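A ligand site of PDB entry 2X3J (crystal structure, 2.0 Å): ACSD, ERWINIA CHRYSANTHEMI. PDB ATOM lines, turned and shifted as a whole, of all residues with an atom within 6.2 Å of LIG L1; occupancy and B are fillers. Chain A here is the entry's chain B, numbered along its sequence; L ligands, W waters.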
ATOM      1  N   HIS A 170      -7.941 -24.791 -21.306  1.00  0.00           N
ATOM      2  CA  HIS A 170      -6.599 -24.410 -20.848  1.00  0.00           C
ATOM      3  C   HIS A 170      -5.868 -25.625 -20.217  1.00  0.00           C
ATOM      4  O   HIS A 170      -6.378 -26.231 -19.284  1.00  0.00           O
ATOM      5  CB  HIS A 170      -6.709 -23.262 -19.834  1.00  0.00           C
ATOM      6  CG  HIS A 170      -5.416 -22.536 -19.579  1.00  0.00           C
ATOM      7  ND1 HIS A 170      -4.263 -23.164 -19.201  1.00  0.00           N
ATOM      8  CD2 HIS A 170      -5.122 -21.214 -19.636  1.00  0.00           C
ATOM      9  CE1 HIS A 170      -3.299 -22.272 -19.046  1.00  0.00           C
ATOM     10  NE2 HIS A 170      -3.802 -21.075 -19.308  1.00  0.00           N
ATOM     11  N   HIS A 173      -4.468 -25.189 -15.933  1.00  0.00           N
ATOM     12  CA  HIS A 173      -5.423 -24.412 -15.181  1.00  0.00           C
ATOM     13  C   HIS A 173      -6.171 -25.401 -14.304  1.00  0.00           C
ATOM     14  O   HIS A 173      -6.501 -26.504 -14.753  1.00  0.00           O
ATOM     15  CB  HIS A 173      -6.384 -23.676 -16.111  1.00  0.00           C
ATOM     16  CG  HIS A 173      -7.144 -22.568 -15.449  1.00  0.00           C
ATOM     17  ND1 HIS A 173      -8.272 -22.786 -14.684  1.00  0.00           N
ATOM     18  CD2 HIS A 173      -6.939 -21.222 -15.443  1.00  0.00           C
ATOM     19  CE1 HIS A 173      -8.719 -21.627 -14.225  1.00  0.00           C
ATOM     20  NE2 HIS A 173      -7.938 -20.666 -14.680  1.00  0.00           N
ATOM     21  N   ILE A 300     -14.983 -17.227 -16.593  1.00  0.00           N
ATOM     22  CA  ILE A 300     -14.423 -18.257 -17.452  1.00  0.00           C
ATOM     23  C   ILE A 300     -12.917 -18.173 -17.248  1.00  0.00           C
ATOM     24  O   ILE A 300     -12.308 -17.093 -17.389  1.00  0.00           O
ATOM     25  CB  ILE A 300     -14.780 -18.030 -18.964  1.00  0.00           C
ATOM     26  CG1 ILE A 300     -16.275 -17.685 -19.176  1.00  0.00           C
ATOM     27  CG2 ILE A 300     -14.277 -19.199 -19.842  1.00  0.00           C
ATOM     28  CD1 ILE A 300     -17.258 -18.730 -18.715  1.00  0.00           C
ATOM     29  N   THR A 301     -12.326 -19.325 -16.915  1.00  0.00           N
ATOM     30  CA  THR A 301     -10.981 -19.409 -16.356  1.00  0.00           C
ATOM     31  C   THR A 301     -10.755 -18.289 -15.319  1.00  0.00           C
ATOM     32  O   THR A 301     -11.474 -18.258 -14.312  1.00  0.00           O
ATOM     33  CB  THR A 301      -9.874 -19.548 -17.445  1.00  0.00           C
ATOM     34  OG1 THR A 301     -10.160 -18.700 -18.560  1.00  0.00           O
ATOM     35  CG2 THR A 301      -9.810 -21.001 -17.928  1.00  0.00           C
ATOM     36  N   ASN A 302      -9.832 -17.373 -15.580  1.00  0.00           N
ATOM     37  CA  ASN A 302      -9.455 -16.352 -14.575  1.00  0.00           C
ATOM     38  C   ASN A 302     -10.353 -15.109 -14.442  1.00  0.00           C
ATOM     39  O   ASN A 302     -10.371 -14.485 -13.386  1.00  0.00           O
ATOM     40  CB  ASN A 302      -8.007 -15.879 -14.790  1.00  0.00           C
ATOM     41  CG  ASN A 302      -6.975 -16.946 -14.459  1.00  0.00           C
ATOM     42  OD1 ASN A 302      -7.297 -18.038 -13.999  1.00  0.00           O
ATOM     43  ND2 ASN A 302      -5.704 -16.605 -14.692  1.00  0.00           N
ATOM     44  N   CYS A 303     -11.076 -14.759 -15.513  1.00  0.00           N
ATOM     45  CA  CYS A 303     -11.795 -13.464 -15.562  1.00  0.00           C
ATOM     46  C   CYS A 303     -13.309 -13.594 -15.719  1.00  0.00           C
ATOM     47  O   CYS A 303     -13.790 -14.487 -16.419  1.00  0.00           O
ATOM     48  CB  CYS A 303     -11.268 -12.607 -16.721  1.00  0.00           C
ATOM     49  SG  CYS A 303      -9.457 -12.540 -16.885  1.00  0.00           S
ATOM     50  N   ARG A 305     -16.128 -12.390 -17.736  1.00  0.00           N
ATOM     51  CA  ARG A 305     -15.915 -12.049 -19.153  1.00  0.00           C
ATOM     52  C   ARG A 305     -16.787 -10.881 -19.656  1.00  0.00           C
ATOM     53  O   ARG A 305     -17.546 -11.000 -20.632  1.00  0.00           O
ATOM     54  CB  ARG A 305     -16.052 -13.301 -20.029  1.00  0.00           C
ATOM     55  CG  ARG A 305     -15.050 -14.408 -19.678  1.00  0.00           C
ATOM     56  CD  ARG A 305     -13.615 -13.956 -19.890  1.00  0.00           C
ATOM     57  NE  ARG A 305     -12.630 -14.955 -19.475  1.00  0.00           N
ATOM     58  CZ  ARG A 305     -11.319 -14.817 -19.636  1.00  0.00           C
ATOM     59  NH1 ARG A 305     -10.485 -15.773 -19.234  1.00  0.00           N
ATOM     60  NH2 ARG A 305     -10.829 -13.715 -20.194  1.00  0.00           N
ATOM     61  N   GLU A 442      -1.114 -10.366 -26.625  1.00  0.00           N
ATOM     62  CA  GLU A 442      -1.203 -11.494 -25.708  1.00  0.00           C
ATOM     63  C   GLU A 442      -1.299 -12.793 -26.520  1.00  0.00           C
ATOM     64  O   GLU A 442      -2.395 -13.349 -26.676  1.00  0.00           O
ATOM     65  CB  GLU A 442      -2.403 -11.324 -24.792  1.00  0.00           C
ATOM     66  CG  GLU A 442      -2.359 -12.230 -23.573  1.00  0.00           C
ATOM     67  CD  GLU A 442      -3.583 -12.070 -22.702  1.00  0.00           C
ATOM     68  OE1 GLU A 442      -4.506 -11.330 -23.098  1.00  0.00           O
ATOM     69  OE2 GLU A 442      -3.626 -12.694 -21.618  1.00  0.00           O
ATOM     70  N   HIS A 444      -1.200 -15.950 -26.551  1.00  0.00           N
ATOM     71  CA  HIS A 444      -1.441 -17.263 -25.992  1.00  0.00           C
ATOM     72  C   HIS A 444      -2.237 -18.096 -26.974  1.00  0.00           C
ATOM     73  O   HIS A 444      -2.671 -17.587 -28.015  1.00  0.00           O
ATOM     74  CB  HIS A 444      -2.124 -17.148 -24.626  1.00  0.00           C
ATOM     75  CG  HIS A 444      -3.483 -16.528 -24.666  1.00  0.00           C
ATOM     76  ND1 HIS A 444      -4.445 -16.879 -25.581  1.00  0.00           N
ATOM     77  CD2 HIS A 444      -4.066 -15.614 -23.840  1.00  0.00           C
ATOM     78  CE1 HIS A 444      -5.554 -16.204 -25.340  1.00  0.00           C
ATOM     79  NE2 HIS A 444      -5.349 -15.424 -24.296  1.00  0.00           N
ATOM     80  N   ASN A 447      -5.584 -16.896 -28.519  1.00  0.00           N
ATOM     81  CA  ASN A 447      -5.501 -15.697 -29.348  1.00  0.00           C
ATOM     82  C   ASN A 447      -4.770 -15.928 -30.659  1.00  0.00           C
ATOM     83  O   ASN A 447      -4.532 -14.974 -31.398  1.00  0.00           O
ATOM     84  CB  ASN A 447      -4.831 -14.525 -28.593  1.00  0.00           C
ATOM     85  CG  ASN A 447      -5.763 -13.879 -27.558  1.00  0.00           C
ATOM     86  OD1 ASN A 447      -6.997 -14.073 -27.605  1.00  0.00           O
ATOM     87  ND2 ASN A 447      -5.188 -13.116 -26.627  1.00  0.00           N
ATOM     88  N   ASP A 464      -7.618 -10.318 -30.649  1.00  0.00           N
ATOM     89  CA  ASP A 464      -8.088  -9.902 -29.331  1.00  0.00           C
ATOM     90  C   ASP A 464      -7.459  -8.599 -28.864  1.00  0.00           C
ATOM     91  O   ASP A 464      -6.553  -8.576 -28.026  1.00  0.00           O
ATOM     92  CB  ASP A 464      -7.966 -11.000 -28.271  1.00  0.00           C
ATOM     93  CG  ASP A 464      -8.871 -10.768 -27.062  1.00  0.00           C
ATOM     94  OD1 ASP A 464      -8.999 -11.709 -26.247  1.00  0.00           O
ATOM     95  OD2 ASP A 464      -9.473  -9.674 -26.966  1.00  0.00           O
ATOM     96  N   GLU A 466      -8.572  -6.338 -26.993  1.00  0.00           N
ATOM     97  CA  GLU A 466      -8.816  -6.037 -25.590  1.00  0.00           C
ATOM     98  C   GLU A 466      -7.595  -6.413 -24.767  1.00  0.00           C
ATOM     99  O   GLU A 466      -7.266  -5.742 -23.785  1.00  0.00           O
ATOM    100  CB  GLU A 466     -10.092  -6.748 -25.096  1.00  0.00           C
ATOM    101  CG  GLU A 466     -10.040  -7.349 -23.675  1.00  0.00           C
ATOM    102  CD  GLU A 466     -11.028  -8.513 -23.476  1.00  0.00           C
ATOM    103  OE1 GLU A 466     -10.985  -9.487 -24.269  1.00  0.00           O
ATOM    104  OE2 GLU A 466     -11.836  -8.466 -22.531  1.00  0.00           O
ATOM    105  N   GLY A 467      -6.903  -7.445 -25.211  1.00  0.00           N
ATOM    106  CA  GLY A 467      -5.651  -7.820 -24.577  1.00  0.00           C
ATOM    107  C   GLY A 467      -4.469  -6.898 -24.821  1.00  0.00           C
ATOM    108  O   GLY A 467      -3.482  -6.946 -24.079  1.00  0.00           O
ATOM    109  N   LYS A 469      -1.742  -4.082 -25.039  1.00  0.00           N
ATOM    110  CA  LYS A 469      -1.211  -3.022 -24.187  1.00  0.00           C
ATOM    111  C   LYS A 469      -0.121  -2.253 -24.911  1.00  0.00           C
ATOM    112  O   LYS A 469       0.435  -2.716 -25.903  1.00  0.00           O
ATOM    113  CB  LYS A 469      -0.683  -3.589 -22.855  1.00  0.00           C
ATOM    114  CG  LYS A 469      -1.689  -4.414 -22.071  1.00  0.00           C
ATOM    115  CD  LYS A 469      -2.945  -3.614 -21.730  1.00  0.00           C
ATOM    116  CE  LYS A 469      -3.832  -4.369 -20.711  1.00  0.00           C
ATOM    117  NZ  LYS A 469      -5.224  -3.853 -20.668  1.00  0.00           N
ATOM    118  N   ARG A 501       4.629 -10.581 -19.924  1.00  0.00           N
ATOM    119  CA  ARG A 501       3.483 -11.170 -20.596  1.00  0.00           C
ATOM    120  C   ARG A 501       3.912 -11.868 -21.911  1.00  0.00           C
ATOM    121  O   ARG A 501       3.515 -13.011 -22.196  1.00  0.00           O
ATOM    122  CB  ARG A 501       2.376 -10.142 -20.854  1.00  0.00           C
ATOM    123  CG  ARG A 501       1.532 -10.426 -22.131  1.00  0.00           C
ATOM    124  CD  ARG A 501       0.347  -9.482 -22.296  1.00  0.00           C
ATOM    125  NE  ARG A 501      -0.597  -9.720 -21.213  1.00  0.00           N
ATOM    126  CZ  ARG A 501      -1.747  -9.074 -21.060  1.00  0.00           C
ATOM    127  NH1 ARG A 501      -2.529  -9.394 -20.021  1.00  0.00           N
ATOM    128  NH2 ARG A 501      -2.109  -8.123 -21.906  1.00  0.00           N
ATOM    129  N   TYR A 504       5.877 -15.062 -21.062  1.00  0.00           N
ATOM    130  CA  TYR A 504       4.972 -16.107 -20.623  1.00  0.00           C
ATOM    131  C   TYR A 504       4.138 -16.632 -21.785  1.00  0.00           C
ATOM    132  O   TYR A 504       4.035 -17.843 -21.964  1.00  0.00           O
ATOM    133  CB  TYR A 504       4.027 -15.630 -19.530  1.00  0.00           C
ATOM    134  CG  TYR A 504       2.845 -16.564 -19.433  1.00  0.00           C
ATOM    135  CD1 TYR A 504       3.010 -17.869 -18.992  1.00  0.00           C
ATOM    136  CD2 TYR A 504       1.576 -16.147 -19.821  1.00  0.00           C
ATOM    137  CE1 TYR A 504       1.939 -18.746 -18.921  1.00  0.00           C
ATOM    138  CE2 TYR A 504       0.488 -17.023 -19.754  1.00  0.00           C
ATOM    139  CZ  TYR A 504       0.689 -18.317 -19.309  1.00  0.00           C
ATOM    140  OH  TYR A 504      -0.373 -19.177 -19.250  1.00  0.00           O
ATOM    141  N   CYS A 505       3.507 -15.746 -22.534  1.00  0.00           N
ATOM    142  CA  CYS A 505       2.604 -16.191 -23.596  1.00  0.00           C
ATOM    143  C   CYS A 505       3.329 -16.947 -24.694  1.00  0.00           C
ATOM    144  O   CYS A 505       2.840 -17.959 -25.128  1.00  0.00           O
ATOM    145  CB  CYS A 505       1.861 -15.012 -24.253  1.00  0.00           C
ATOM    146  SG  CYS A 505       0.568 -14.330 -23.233  1.00  0.00           S
ATOM    147  N   ASN A 509       3.125 -20.606 -22.388  1.00  0.00           N
ATOM    148  CA  ASN A 509       1.744 -20.963 -22.688  1.00  0.00           C
ATOM    149  C   ASN A 509       1.625 -21.599 -24.080  1.00  0.00           C
ATOM    150  O   ASN A 509       0.850 -22.517 -24.269  1.00  0.00           O
ATOM    151  CB  ASN A 509       0.859 -19.720 -22.537  1.00  0.00           C
ATOM    152  CG  ASN A 509      -0.564 -19.928 -23.015  1.00  0.00           C
ATOM    153  OD1 ASN A 509      -0.806 -20.225 -24.212  1.00  0.00           O
ATOM    154  ND2 ASN A 509      -1.518 -19.719 -22.116  1.00  0.00           N
ATOM    155  N   LYS A 563       3.243 -17.006 -15.882  1.00  0.00           N
ATOM    156  CA  LYS A 563       2.030 -16.613 -15.178  1.00  0.00           C
ATOM    157  C   LYS A 563       1.465 -17.767 -14.341  1.00  0.00           C
ATOM    158  O   LYS A 563       1.445 -18.918 -14.782  1.00  0.00           O
ATOM    159  CB  LYS A 563       1.004 -16.091 -16.185  1.00  0.00           C
ATOM    160  CG  LYS A 563      -0.328 -15.685 -15.589  1.00  0.00           C
ATOM    161  CD  LYS A 563      -1.131 -14.936 -16.627  1.00  0.00           C
ATOM    162  CE  LYS A 563      -2.613 -14.954 -16.307  1.00  0.00           C
ATOM    163  NZ  LYS A 563      -3.344 -14.100 -17.293  1.00  0.00           N
ATOM    164  N   ASN A 565      -1.608 -19.413 -12.912  1.00  0.00           N
ATOM    165  CA  ASN A 565      -3.078 -19.503 -12.929  1.00  0.00           C
ATOM    166  C   ASN A 565      -3.698 -20.048 -11.635  1.00  0.00           C
ATOM    167  O   ASN A 565      -4.725 -19.540 -11.191  1.00  0.00           O
ATOM    168  CB  ASN A 565      -3.587 -20.283 -14.150  1.00  0.00           C
ATOM    169  CG  ASN A 565      -3.240 -19.604 -15.446  1.00  0.00           C
ATOM    170  OD1 ASN A 565      -3.311 -18.378 -15.575  1.00  0.00           O
ATOM    171  ND2 ASN A 565      -2.854 -20.405 -16.415  1.00  0.00           N
HETATM  172  C1  LIG L   1      -3.451 -17.424 -19.406  1.00  0.00           C
HETATM  173  O1  LIG L   1      -3.093 -16.217 -19.462  1.00  0.00           O
HETATM  174  O2  LIG L   1      -2.705 -18.427 -19.451  1.00  0.00           O
HETATM  175  C2  LIG L   1      -4.953 -17.742 -19.284  1.00  0.00           C
HETATM  176  C3  LIG L   1      -6.376 -10.971 -19.986  1.00  0.00           C
HETATM  177  N1  LIG L   1      -6.306  -9.909 -21.006  1.00  0.00           N
HETATM  178  O3  LIG L   1      -5.444 -15.665 -18.076  1.00  0.00           O
HETATM  179  C4  LIG L   1      -7.289 -17.158 -18.717  1.00  0.00           C
HETATM  180  O4  LIG L   1      -7.785 -16.854 -17.608  1.00  0.00           O
HETATM  181  C5  LIG L   1      -7.230 -12.110 -20.536  1.00  0.00           C
HETATM  182  N2  LIG L   1      -6.449 -13.366 -20.636  1.00  0.00           N
HETATM  183  C6  LIG L   1      -6.981 -14.527 -20.268  1.00  0.00           C
HETATM  184  C7  LIG L   1      -5.922 -16.549 -19.100  1.00  0.00           C
HETATM  185  O5  LIG L   1      -8.132 -14.642 -19.810  1.00  0.00           O
HETATM  186  C8  LIG L   1      -6.053 -15.753 -20.421  1.00  0.00           C
HETATM  187  O6  LIG L   1      -7.819 -17.933 -19.532  1.00  0.00           O
HETATM  188  P1  LG2 L   2     -11.889 -13.500 -27.803  1.00  0.00           P
HETATM  189  O1  LG2 L   2     -10.542 -14.207 -27.872  1.00  0.00           O
HETATM  190  O2  LG2 L   2     -12.957 -14.267 -28.546  1.00  0.00           O
HETATM  191  O3  LG2 L   2     -11.867 -12.011 -28.031  1.00  0.00           O
HETATM  192  P2  LG2 L   2     -11.737 -13.231 -24.887  1.00  0.00           P
HETATM  193  O4  LG2 L   2     -12.728 -13.672 -23.823  1.00  0.00           O
HETATM  194  O5  LG2 L   2     -11.416 -11.763 -24.903  1.00  0.00           O
HETATM  195  O6  LG2 L   2     -12.438 -13.669 -26.273  1.00  0.00           O
HETATM  196  P3  LG2 L   2      -9.164 -13.960 -23.775  1.00  0.00           P
HETATM  197  O7  LG2 L   2      -7.906 -13.888 -24.623  1.00  0.00           O
HETATM  198  O8  LG2 L   2      -9.500 -12.896 -22.733  1.00  0.00           O
HETATM  199  O9  LG2 L   2     -10.402 -14.117 -24.824  1.00  0.00           O
HETATM  200  O10 LG2 L   2      -9.216 -15.356 -22.942  1.00  0.00           O
HETATM  201  C1  LG2 L   2      -8.905 -16.622 -23.496  1.00  0.00           C
HETATM  202  C2  LG2 L   2     -10.152 -17.519 -23.506  1.00  0.00           C
HETATM  203  O11 LG2 L   2      -9.728 -18.744 -24.114  1.00  0.00           O
HETATM  204  C3  LG2 L   2     -10.635 -17.934 -22.118  1.00  0.00           C
HETATM  205  O12 LG2 L   2     -12.013 -18.346 -22.182  1.00  0.00           O
HETATM  206  C4  LG2 L   2      -9.751 -19.137 -21.804  1.00  0.00           C
HETATM  207  O13 LG2 L   2     -10.356 -20.036 -20.876  1.00  0.00           O
HETATM  208  C5  LG2 L   2      -9.632 -19.818 -23.171  1.00  0.00           C
HETATM  209  N1  LG2 L   2      -8.373 -20.598 -23.334  1.00  0.00           N
HETATM  210  C6  LG2 L   2      -8.317 -21.909 -23.654  1.00  0.00           C
HETATM  211  N2  LG2 L   2      -7.037 -22.349 -23.743  1.00  0.00           N
HETATM  212  C7  LG2 L   2      -6.239 -21.292 -23.461  1.00  0.00           C
HETATM  213  C8  LG2 L   2      -4.791 -21.060 -23.381  1.00  0.00           C
HETATM  214  N3  LG2 L   2      -3.952 -22.092 -23.606  1.00  0.00           N
HETATM  215  N4  LG2 L   2      -4.353 -19.812 -23.067  1.00  0.00           N
HETATM  216  C9  LG2 L   2      -5.198 -18.793 -22.822  1.00  0.00           C
HETATM  217  N5  LG2 L   2      -6.545 -18.928 -22.870  1.00  0.00           N
HETATM  218  C10 LG2 L   2      -7.126 -20.138 -23.188  1.00  0.00           C
HETATM  219  O   HOH W   1      -8.351 -10.263 -23.679  1.00  0.00           O
HETATM  220  O   HOH W   2      -1.951 -14.188 -20.301  1.00  0.00           O
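Water W2 lies within hydrogen-bond range of an oxygen (O1) of LIG L1 (2.5 Å), the side-chain carboxylate of Glu 442 (2.6 Å) and the side-chain amino group of Lys 563 (3.3 Å).
Water W1 lies within hydrogen-bond range of the side-chain carboxylate of Glu 466, an oxygen (O8) of LG2 L2 and a nitrogen (N1) of LIG L1.
O of Ile 300 is in hydrogen-bond range of NH1 of Arg 305, at 2.9 Å.
OE2 of Glu 442 lies within salt-bridge range of NH1 of Arg 501.
A ring nitrogen (ND1) of His 444 is in hydrogen-bond range of the backbone NH of Asn 447, 3.2 Å away.
The side-chain amide nitrogen (ND2) of Asn 302 sits at hydrogen-bond distance from the side-chain amide oxygen (OD1) of Asn 565, 3.1 Å away.
The side-chain hydroxyl (OG1) of Thr 301 sits at hydrogen-bond distance from the guanidinium group (NH1) of Arg 305 (3.0 Å).
NE2 of His 173 lies within hydrogen-bond range of OD1 of Asn 302 (2.8 Å).
O of Arg 501 lies close to SG of Cys 505, at 3.4 Å.
O of Tyr 504 is in hydrogen-bond range of N of Asn 509.
An oxygen (O8) of LG2 L2 is in salt-bridge range of the guanidinium group (NH2) of Arg 305 (3.0 Å).
A ring nitrogen (NE2) of His 170 is in hydrogen-bond range of an oxygen (O2) of LIG L1, at 2.9 Å.
OH of Tyr 504 is in hydrogen-bond range of O2 of LIG L1, 2.5 Å away.
NE2 of His 444 lies close to O7 of LG2 L2 (3.0 Å).
The guanidinium group (NH1) of Arg 305 lies within salt-bridge range of an oxygen (O4) of LIG L1, 3.3 Å away.
The side-chain carboxylate (OE1) of Glu 442 lies within salt-bridge range of a nitrogen (N1) of LIG L1 (3.1 Å).
O1 of LIG L1 lies within salt-bridge range of NZ of Lys 563 (3.0 Å).
ND2 of Asn 509 lies within hydrogen-bond range of O2 of LIG L1.
O13 of LG2 L2 is in hydrogen-bond range of OG1 of Thr 301, 2.7 Å away.
The side-chain amide nitrogen (ND2) of Asn 509 lies within hydrogen-bond range of a nitrogen (N4) of LG2 L2 (3.0 Å).
OE1 of Glu 466 sits close to O5 of LG2 L2 (2.4 Å).
The side-chain hydroxyl (OG1) of Thr 301 is in hydrogen-bond range of an oxygen (O6) of LIG L1, at 2.6 Å.
The backbone NH (N) of Asn 302 sits at hydrogen-bond distance from an oxygen (O4) of LIG L1, 2.9 Å away.
SG of Cys 303 touches O5 of LIG L1, at 3.8 Å.
NE2 of His 444 touches C8 of LIG L1, 3.95 Å away.
Arg 501 touches LIG L1.
Asn 565 touches LIG L1 (ND2 to O2, 3.6 Å).
Hydrophobic or aromatic side chains within 4 Å of LIG L1: His 170, His 444 and Tyr 504.
The nearest printed residue that does not touch LIG L1 is Gly 467 (4.2 Å).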
